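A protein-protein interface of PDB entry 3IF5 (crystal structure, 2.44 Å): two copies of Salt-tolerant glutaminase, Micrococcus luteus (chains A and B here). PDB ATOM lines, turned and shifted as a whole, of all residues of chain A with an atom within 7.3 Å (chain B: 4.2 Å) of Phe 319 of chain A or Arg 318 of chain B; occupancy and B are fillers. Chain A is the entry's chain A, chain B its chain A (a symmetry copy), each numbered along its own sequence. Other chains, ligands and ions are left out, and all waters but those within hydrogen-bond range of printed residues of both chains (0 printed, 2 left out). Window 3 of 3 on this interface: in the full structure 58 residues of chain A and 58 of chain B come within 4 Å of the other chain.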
ATOM      1  N   GLY A 314      18.944 -28.331 -19.644  1.00  0.00           N
ATOM      2  CA  GLY A 314      18.522 -27.598 -20.825  1.00  0.00           C
ATOM      3  C   GLY A 314      19.527 -26.575 -21.322  1.00  0.00           C
ATOM      4  O   GLY A 314      19.397 -26.061 -22.436  1.00  0.00           O
ATOM      5  N   THR A 315      20.532 -26.268 -20.505  1.00  0.00           N
ATOM      6  CA  THR A 315      21.537 -25.299 -20.917  1.00  0.00           C
ATOM      7  C   THR A 315      22.373 -25.892 -22.049  1.00  0.00           C
ATOM      8  O   THR A 315      23.127 -25.177 -22.714  1.00  0.00           O
ATOM      9  CB  THR A 315      22.448 -24.898 -19.742  1.00  0.00           C
ATOM     10  OG1 THR A 315      21.646 -24.410 -18.663  1.00  0.00           O
ATOM     11  CG2 THR A 315      23.405 -23.800 -20.166  1.00  0.00           C
ATOM     12  N   ALA A 316      22.235 -27.200 -22.273  1.00  0.00           N
ATOM     13  CA  ALA A 316      22.966 -27.867 -23.353  1.00  0.00           C
ATOM     14  C   ALA A 316      22.606 -27.179 -24.673  1.00  0.00           C
ATOM     15  O   ALA A 316      23.350 -27.252 -25.650  1.00  0.00           O
ATOM     16  CB  ALA A 316      22.595 -29.355 -23.418  1.00  0.00           C
ATOM     17  N   VAL A 317      21.448 -26.519 -24.691  1.00  0.00           N
ATOM     18  CA  VAL A 317      20.973 -25.798 -25.861  1.00  0.00           C
ATOM     19  C   VAL A 317      21.287 -24.309 -25.673  1.00  0.00           C
ATOM     20  O   VAL A 317      20.558 -23.597 -24.982  1.00  0.00           O
ATOM     21  CB  VAL A 317      19.444 -25.973 -26.037  1.00  0.00           C
ATOM     22  CG1 VAL A 317      18.944 -25.098 -27.172  1.00  0.00           C
ATOM     23  CG2 VAL A 317      19.115 -27.442 -26.313  1.00  0.00           C
ATOM     24  N   ARG A 318      22.377 -23.850 -26.281  1.00  0.00           N
ATOM     25  CA  ARG A 318      22.799 -22.453 -26.178  1.00  0.00           C
ATOM     26  C   ARG A 318      21.701 -21.516 -26.687  1.00  0.00           C
ATOM     27  O   ARG A 318      21.412 -20.491 -26.071  1.00  0.00           O
ATOM     28  CB  ARG A 318      24.095 -22.248 -26.968  1.00  0.00           C
ATOM     29  CG  ARG A 318      24.846 -20.956 -26.666  1.00  0.00           C
ATOM     30  CD  ARG A 318      26.197 -20.942 -27.396  1.00  0.00           C
ATOM     31  NE  ARG A 318      26.934 -19.688 -27.238  1.00  0.00           N
ATOM     32  CZ  ARG A 318      27.488 -19.270 -26.102  1.00  0.00           C
ATOM     33  NH1 ARG A 318      27.399 -19.996 -25.005  1.00  0.00           N
ATOM     34  NH2 ARG A 318      28.138 -18.114 -26.064  1.00  0.00           N
ATOM     35  N   PHE A 319      21.098 -21.873 -27.817  1.00  0.00           N
ATOM     36  CA  PHE A 319      20.008 -21.091 -28.398  1.00  0.00           C
ATOM     37  C   PHE A 319      19.508 -21.668 -29.717  1.00  0.00           C
ATOM     38  O   PHE A 319      20.260 -22.288 -30.476  1.00  0.00           O
ATOM     39  CB  PHE A 319      20.415 -19.630 -28.616  1.00  0.00           C
ATOM     40  CG  PHE A 319      21.516 -19.447 -29.617  1.00  0.00           C
ATOM     41  CD1 PHE A 319      22.841 -19.681 -29.269  1.00  0.00           C
ATOM     42  CD2 PHE A 319      21.232 -19.028 -30.909  1.00  0.00           C
ATOM     43  CE1 PHE A 319      23.871 -19.500 -30.202  1.00  0.00           C
ATOM     44  CE2 PHE A 319      22.252 -18.843 -31.848  1.00  0.00           C
ATOM     45  CZ  PHE A 319      23.571 -19.078 -31.494  1.00  0.00           C
ATOM     46  N   VAL A 320      18.223 -21.461 -29.974  1.00  0.00           N
ATOM     47  CA  VAL A 320      17.596 -21.941 -31.191  1.00  0.00           C
ATOM     48  C   VAL A 320      17.262 -20.714 -32.032  1.00  0.00           C
ATOM     49  O   VAL A 320      16.573 -19.807 -31.562  1.00  0.00           O
ATOM     50  CB  VAL A 320      16.296 -22.710 -30.871  1.00  0.00           C
ATOM     51  CG1 VAL A 320      15.758 -23.367 -32.127  1.00  0.00           C
ATOM     52  CG2 VAL A 320      16.558 -23.747 -29.786  1.00  0.00           C
ATOM     53  N   GLU A 321      17.759 -20.674 -33.266  1.00  0.00           N
ATOM     54  CA  GLU A 321      17.508 -19.537 -34.150  1.00  0.00           C
ATOM     55  C   GLU A 321      16.743 -19.896 -35.410  1.00  0.00           C
ATOM     56  O   GLU A 321      17.272 -20.565 -36.296  1.00  0.00           O
ATOM     57  CB  GLU A 321      18.823 -18.884 -34.578  1.00  0.00           C
ATOM     58  CG  GLU A 321      19.611 -18.242 -33.464  1.00  0.00           C
ATOM     59  CD  GLU A 321      18.878 -17.097 -32.804  1.00  0.00           C
ATOM     60  OE1 GLU A 321      18.508 -16.139 -33.520  1.00  0.00           O
ATOM     61  OE2 GLU A 321      18.678 -17.149 -31.570  1.00  0.00           O
ATOM     62  N   VAL A 327      16.549 -23.635 -39.336  1.00  0.00           N
ATOM     63  CA  VAL A 327      16.737 -23.451 -37.906  1.00  0.00           C
ATOM     64  C   VAL A 327      18.195 -23.690 -37.528  1.00  0.00           C
ATOM     65  O   VAL A 327      18.827 -24.637 -37.998  1.00  0.00           O
ATOM     66  CB  VAL A 327      15.859 -24.434 -37.103  1.00  0.00           C
ATOM     67  CG1 VAL A 327      15.880 -24.067 -35.628  1.00  0.00           C
ATOM     68  CG2 VAL A 327      14.443 -24.423 -37.644  1.00  0.00           C
ATOM     69  N   PHE A 328      18.727 -22.810 -36.687  1.00  0.00           N
ATOM     70  CA  PHE A 328      20.100 -22.936 -36.224  1.00  0.00           C
ATOM     71  C   PHE A 328      20.057 -23.381 -34.769  1.00  0.00           C
ATOM     72  O   PHE A 328      19.473 -22.710 -33.915  1.00  0.00           O
ATOM     73  CB  PHE A 328      20.843 -21.603 -36.331  1.00  0.00           C
ATOM     74  CG  PHE A 328      20.997 -21.108 -37.739  1.00  0.00           C
ATOM     75  CD1 PHE A 328      19.941 -20.485 -38.396  1.00  0.00           C
ATOM     76  CD2 PHE A 328      22.201 -21.285 -38.420  1.00  0.00           C
ATOM     77  CE1 PHE A 328      20.078 -20.045 -39.710  1.00  0.00           C
ATOM     78  CE2 PHE A 328      22.349 -20.850 -39.733  1.00  0.00           C
ATOM     79  CZ  PHE A 328      21.285 -20.227 -40.380  1.00  0.00           C
ATOM     80  N   LEU A 329      20.678 -24.519 -34.491  1.00  0.00           N
ATOM     81  CA  LEU A 329      20.694 -25.052 -33.142  1.00  0.00           C
ATOM     82  C   LEU A 329      22.120 -25.107 -32.615  1.00  0.00           C
ATOM     83  O   LEU A 329      22.946 -25.889 -33.097  1.00  0.00           O
ATOM     84  CB  LEU A 329      20.067 -26.449 -33.139  1.00  0.00           C
ATOM     85  CG  LEU A 329      19.714 -27.069 -31.790  1.00  0.00           C
ATOM     86  CD1 LEU A 329      18.836 -26.118 -30.992  1.00  0.00           C
ATOM     87  CD2 LEU A 329      18.992 -28.381 -32.024  1.00  0.00           C
ATOM     88  N   HIS A 330      22.411 -24.262 -31.633  1.00  0.00           N
ATOM     89  CA  HIS A 330      23.742 -24.225 -31.038  1.00  0.00           C
ATOM     90  C   HIS A 330      23.771 -24.927 -29.684  1.00  0.00           C
ATOM     91  O   HIS A 330      22.955 -24.652 -28.804  1.00  0.00           O
ATOM     92  CB  HIS A 330      24.222 -22.778 -30.883  1.00  0.00           C
ATOM     93  CG  HIS A 330      24.629 -22.135 -32.173  1.00  0.00           C
ATOM     94  ND1 HIS A 330      23.732 -21.843 -33.179  1.00  0.00           N
ATOM     95  CD2 HIS A 330      25.843 -21.730 -32.623  1.00  0.00           C
ATOM     96  CE1 HIS A 330      24.374 -21.290 -34.194  1.00  0.00           C
ATOM     97  NE2 HIS A 330      25.656 -21.211 -33.880  1.00  0.00           N
ATOM     98  N   LEU A 331      24.729 -25.836 -29.529  1.00  0.00           N
ATOM     99  CA  LEU A 331      24.888 -26.603 -28.301  1.00  0.00           C
ATOM    100  C   LEU A 331      26.142 -26.181 -27.537  1.00  0.00           C
ATOM    101  O   LEU A 331      27.031 -25.539 -28.099  1.00  0.00           O
ATOM    102  CB  LEU A 331      24.953 -28.095 -28.630  1.00  0.00           C
ATOM    103  CG  LEU A 331      23.776 -28.637 -29.448  1.00  0.00           C
ATOM    104  CD1 LEU A 331      23.959 -30.130 -29.669  1.00  0.00           C
ATOM    105  CD2 LEU A 331      22.468 -28.361 -28.731  1.00  0.00           C
ATOM    106  N   GLN A 332      26.216 -26.555 -26.261  1.00  0.00           N
ATOM    107  CA  GLN A 332      27.358 -26.202 -25.420  1.00  0.00           C
ATOM    108  C   GLN A 332      27.488 -27.090 -24.180  1.00  0.00           C
ATOM    109  O   GLN A 332      26.577 -27.847 -23.845  1.00  0.00           O
ATOM    110  CB  GLN A 332      27.227 -24.746 -24.976  1.00  0.00           C
ATOM    111  CG  GLN A 332      26.068 -24.516 -24.015  1.00  0.00           C
ATOM    112  CD  GLN A 332      25.804 -23.047 -23.780  1.00  0.00           C
ATOM    113  OE1 GLN A 332      26.679 -22.217 -24.005  1.00  0.00           O
ATOM    114  NE2 GLN A 332      24.602 -22.717 -23.316  1.00  0.00           N
ATOM    115  N   ASN A 410      25.186 -26.830 -34.474  1.00  0.00           N
ATOM    116  CA  ASN A 410      26.463 -26.199 -34.172  1.00  0.00           C
ATOM    117  C   ASN A 410      27.054 -26.768 -32.885  1.00  0.00           C
ATOM    118  O   ASN A 410      26.520 -26.552 -31.796  1.00  0.00           O
ATOM    119  CB  ASN A 410      26.285 -24.688 -34.039  1.00  0.00           C
ATOM    120  CG  ASN A 410      27.604 -23.953 -33.934  1.00  0.00           C
ATOM    121  OD1 ASN A 410      28.349 -24.124 -32.970  1.00  0.00           O
ATOM    122  ND2 ASN A 410      27.899 -23.130 -34.929  1.00  0.00           N
ATOM    123  N   ARG A 413      30.516 -24.767 -29.494  1.00  0.00           N
ATOM    124  CA  ARG A 413      30.524 -24.440 -28.069  1.00  0.00           C
ATOM    125  C   ARG A 413      30.522 -25.656 -27.137  1.00  0.00           C
ATOM    126  O   ARG A 413      30.617 -25.512 -25.921  1.00  0.00           O
ATOM    127  CB  ARG A 413      29.322 -23.549 -27.740  1.00  0.00           C
ATOM    128  CG  ARG A 413      29.391 -22.166 -28.354  1.00  0.00           C
ATOM    129  CD  ARG A 413      30.462 -21.336 -27.692  1.00  0.00           C
ATOM    130  NE  ARG A 413      30.540 -19.994 -28.254  1.00  0.00           N
ATOM    131  CZ  ARG A 413      31.334 -19.037 -27.787  1.00  0.00           C
ATOM    132  NH1 ARG A 413      32.111 -19.282 -26.751  1.00  0.00           N
ATOM    133  NH2 ARG A 413      31.349 -17.844 -28.364  1.00  0.00           N
ATOM    134  N   THR B 315      30.399 -23.710 -17.958  1.00  0.00           N
ATOM    135  CA  THR B 315      29.379 -23.275 -18.902  1.00  0.00           C
ATOM    136  C   THR B 315      28.537 -22.173 -18.259  1.00  0.00           C
ATOM    137  O   THR B 315      27.769 -21.491 -18.942  1.00  0.00           O
ATOM    138  CB  THR B 315      28.476 -24.444 -19.335  1.00  0.00           C
ATOM    139  OG1 THR B 315      29.284 -25.496 -19.870  1.00  0.00           O
ATOM    140  CG2 THR B 315      27.503 -23.990 -20.408  1.00  0.00           C
ATOM    141  N   ALA B 316      28.688 -21.995 -16.945  1.00  0.00           N
ATOM    142  CA  ALA B 316      27.953 -20.948 -16.232  1.00  0.00           C
ATOM    143  C   ALA B 316      28.292 -19.600 -16.875  1.00  0.00           C
ATOM    144  O   ALA B 316      27.538 -18.635 -16.759  1.00  0.00           O
ATOM    145  CB  ALA B 316      28.338 -20.933 -14.747  1.00  0.00           C
ATOM    146  N   VAL B 317      29.442 -19.546 -17.546  1.00  0.00           N
ATOM    147  CA  VAL B 317      29.897 -18.346 -18.229  1.00  0.00           C
ATOM    148  C   VAL B 317      29.569 -18.483 -19.721  1.00  0.00           C
ATOM    149  O   VAL B 317      30.298 -19.140 -20.464  1.00  0.00           O
ATOM    150  CB  VAL B 317      31.427 -18.160 -18.063  1.00  0.00           C
ATOM    151  CG1 VAL B 317      31.906 -16.989 -18.903  1.00  0.00           C
ATOM    152  CG2 VAL B 317      31.769 -17.934 -16.589  1.00  0.00           C
ATOM    153  N   ARG B 318      28.468 -17.871 -20.146  1.00  0.00           N
ATOM    154  CA  ARG B 318      28.033 -17.927 -21.541  1.00  0.00           C
ATOM    155  C   ARG B 318      29.116 -17.373 -22.471  1.00  0.00           C
ATOM    156  O   ARG B 318      29.400 -17.949 -23.520  1.00  0.00           O
ATOM    157  CB  ARG B 318      26.727 -17.145 -21.704  1.00  0.00           C
ATOM    158  CG  ARG B 318      25.965 -17.408 -22.999  1.00  0.00           C
ATOM    159  CD  ARG B 318      24.606 -16.692 -22.972  1.00  0.00           C
ATOM    160  NE  ARG B 318      23.858 -16.813 -24.223  1.00  0.00           N
ATOM    161  CZ  ARG B 318      23.311 -17.938 -24.677  1.00  0.00           C
ATOM    162  NH1 ARG B 318      23.419 -19.061 -23.992  1.00  0.00           N
ATOM    163  NH2 ARG B 318      22.649 -17.942 -25.826  1.00  0.00           N
ATOM    164  N   PHE B 319      29.711 -16.250 -22.079  1.00  0.00           N
ATOM    165  CA  PHE B 319      30.786 -15.630 -22.851  1.00  0.00           C
ATOM    166  C   PHE B 319      31.279 -14.327 -22.231  1.00  0.00           C
ATOM    167  O   PHE B 319      30.525 -13.600 -21.577  1.00  0.00           O
ATOM    168  CB  PHE B 319      30.361 -15.364 -24.298  1.00  0.00           C
ATOM    169  CG  PHE B 319      29.249 -14.368 -24.434  1.00  0.00           C
ATOM    170  CD1 PHE B 319      27.929 -14.739 -24.199  1.00  0.00           C
ATOM    171  CD2 PHE B 319      29.515 -13.060 -24.809  1.00  0.00           C
ATOM    172  CE1 PHE B 319      26.888 -13.811 -24.335  1.00  0.00           C
ATOM    173  CE2 PHE B 319      28.483 -12.126 -24.949  1.00  0.00           C
ATOM    174  CZ  PHE B 319      27.170 -12.502 -24.714  1.00  0.00           C
ATOM    175  N   HIS B 330      28.384 -12.537 -19.540  1.00  0.00           N
ATOM    176  CA  HIS B 330      27.059 -13.145 -19.585  1.00  0.00           C
ATOM    177  C   HIS B 330      27.051 -14.524 -18.932  1.00  0.00           C
ATOM    178  O   HIS B 330      27.873 -15.385 -19.247  1.00  0.00           O
ATOM    179  CB  HIS B 330      26.565 -13.253 -21.032  1.00  0.00           C
ATOM    180  CG  HIS B 330      26.138 -11.945 -21.623  1.00  0.00           C
ATOM    181  ND1 HIS B 330      27.022 -10.919 -21.887  1.00  0.00           N
ATOM    182  CD2 HIS B 330      24.915 -11.493 -21.999  1.00  0.00           C
ATOM    183  CE1 HIS B 330      26.363  -9.892 -22.397  1.00  0.00           C
ATOM    184  NE2 HIS B 330      25.083 -10.217 -22.474  1.00  0.00           N
ATOM    185  N   GLN B 332      24.659 -18.030 -17.405  1.00  0.00           N
ATOM    186  CA  GLN B 332      23.522 -18.869 -17.776  1.00  0.00           C
ATOM    187  C   GLN B 332      23.414 -20.141 -16.932  1.00  0.00           C
ATOM    188  O   GLN B 332      24.337 -20.494 -16.197  1.00  0.00           O
ATOM    189  CB  GLN B 332      23.642 -19.259 -19.248  1.00  0.00           C
ATOM    190  CG  GLN B 332      24.809 -20.198 -19.525  1.00  0.00           C
ATOM    191  CD  GLN B 332      25.059 -20.377 -21.004  1.00  0.00           C
ATOM    192  OE1 GLN B 332      24.173 -20.131 -21.816  1.00  0.00           O
ATOM    193  NE2 GLN B 332      26.262 -20.817 -21.363  1.00  0.00           N
ATOM    194  N   ARG B 413      20.307 -14.780 -19.029  1.00  0.00           N
ATOM    195  CA  ARG B 413      20.311 -16.192 -19.408  1.00  0.00           C
ATOM    196  C   ARG B 413      20.335 -17.167 -18.226  1.00  0.00           C
ATOM    197  O   ARG B 413      20.251 -18.379 -18.414  1.00  0.00           O
ATOM    198  CB  ARG B 413      21.506 -16.476 -20.323  1.00  0.00           C
ATOM    199  CG  ARG B 413      21.416 -15.814 -21.682  1.00  0.00           C
ATOM    200  CD  ARG B 413      20.343 -16.456 -22.524  1.00  0.00           C
ATOM    201  NE  ARG B 413      20.245 -15.846 -23.844  1.00  0.00           N
ATOM    202  CZ  ARG B 413      19.445 -16.288 -24.809  1.00  0.00           C
ATOM    203  NH1 ARG B 413      18.682 -17.340 -24.594  1.00  0.00           N
ATOM    204  NH2 ARG B 413      19.412 -15.667 -25.980  1.00  0.00           N
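The backbone carbonyl oxygen (O) of Arg 318 of chain A is in hydrogen-bond range of the guanidinium group (NH2) of Arg 318 of chain B, 2.8 Å away. OE1 of Gln 332 of chain A lies within hydrogen-bond range of NE2 of Gln 332 of chain B (3.0 Å).
O of Thr 315 of chain A is in hydrogen-bond range of NE2 of Gln 332 of chain A (2.9 Å). The backbone NH (N) of Gln 332 of chain A sits at hydrogen-bond distance from the backbone carbonyl oxygen (O) of Ala 316 of chain A (3.0 Å). The backbone NH (N) of Arg 318 of chain A is in hydrogen-bond range of the backbone carbonyl oxygen (O) of His 330 of chain A, at 2.7 Å. NH1 of Arg 318 of chain A lies within hydrogen-bond range of OE1 of Gln 332 of chain A (2.5 Å). The backbone NH (N) of His 330 of chain A is in hydrogen-bond range of the backbone carbonyl oxygen (O) of Phe 319 of chain A, at 3.1 Å. The backbone carbonyl oxygen (O) of Thr 315 of chain B lies within hydrogen-bond range of the side-chain amide nitrogen (NE2) of Gln 332 of chain B, at 2.9 Å.
Arg 318 of chain A touches its own counterpart, Arg 318 of chain B. Arg 318 of chain A touches Phe 319 of chain B, and with the chains exchanged Phe 319 of chain A touches Arg 318 of chain B. Arg 318 of chain A touches Gln 332 of chain B, and with the chains exchanged Gln 332 of chain A touches Arg 318 of chain B. Gln 332 of chain A touches its own counterpart, Gln 332 of chain B. Positions printed for both chains: 315, 316, 317, 318, 319, 330, 332 and 413.
Printed residues of chain B within 4 Å of Thr 315 of chain A: Gln 332. Printed residues of chain A within 4 Å of Gln 332 of chain B: Thr 315, Arg 318 and Gln 332. Of the printed residues of chain B, Arg 318 of chain A touches Arg 318, Phe 319 and Gln 332. Val 320 of chain A touches none of the printed residues of chain B. Leu 331 of chain A touches none of the printed residues of chain B. The nearest printed residue of chain B that does not touch Phe 319 of chain A is Arg 413 of chain B (4.9 Å). The nearest residue of chain A that does not touch Arg 318 of chain B is Arg 413 of chain A (4.4 Å).
Hydrophobic or aromatic side chains of chain A within 4 Å of the printed part of chain B: Phe 319. Hydrophobic or aromatic side chains of chain B within 4 Å of the printed part of chain A: Phe 319. Along chain B the printed residues that touch a printed residue of chain A span positions 315 to 332.
Thr 315 of chain A touches Gln 332 of chain B (CG2 to CD, 3.9 Å). CD1 of Phe 319 of chain B touches NH2 of Arg 318 of chain A, 3.9 Å away. Gln 332 of chain B touches Arg 318 of chain A. Phe 319 of chain A touches Arg 318 of chain B. CD of Gln 332 of chain A touches CG2 of Thr 315 of chain B (3.9 Å). Gln 332 of chain A touches Arg 318 of chain B (NE2 to NH1, 3.9 Å).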
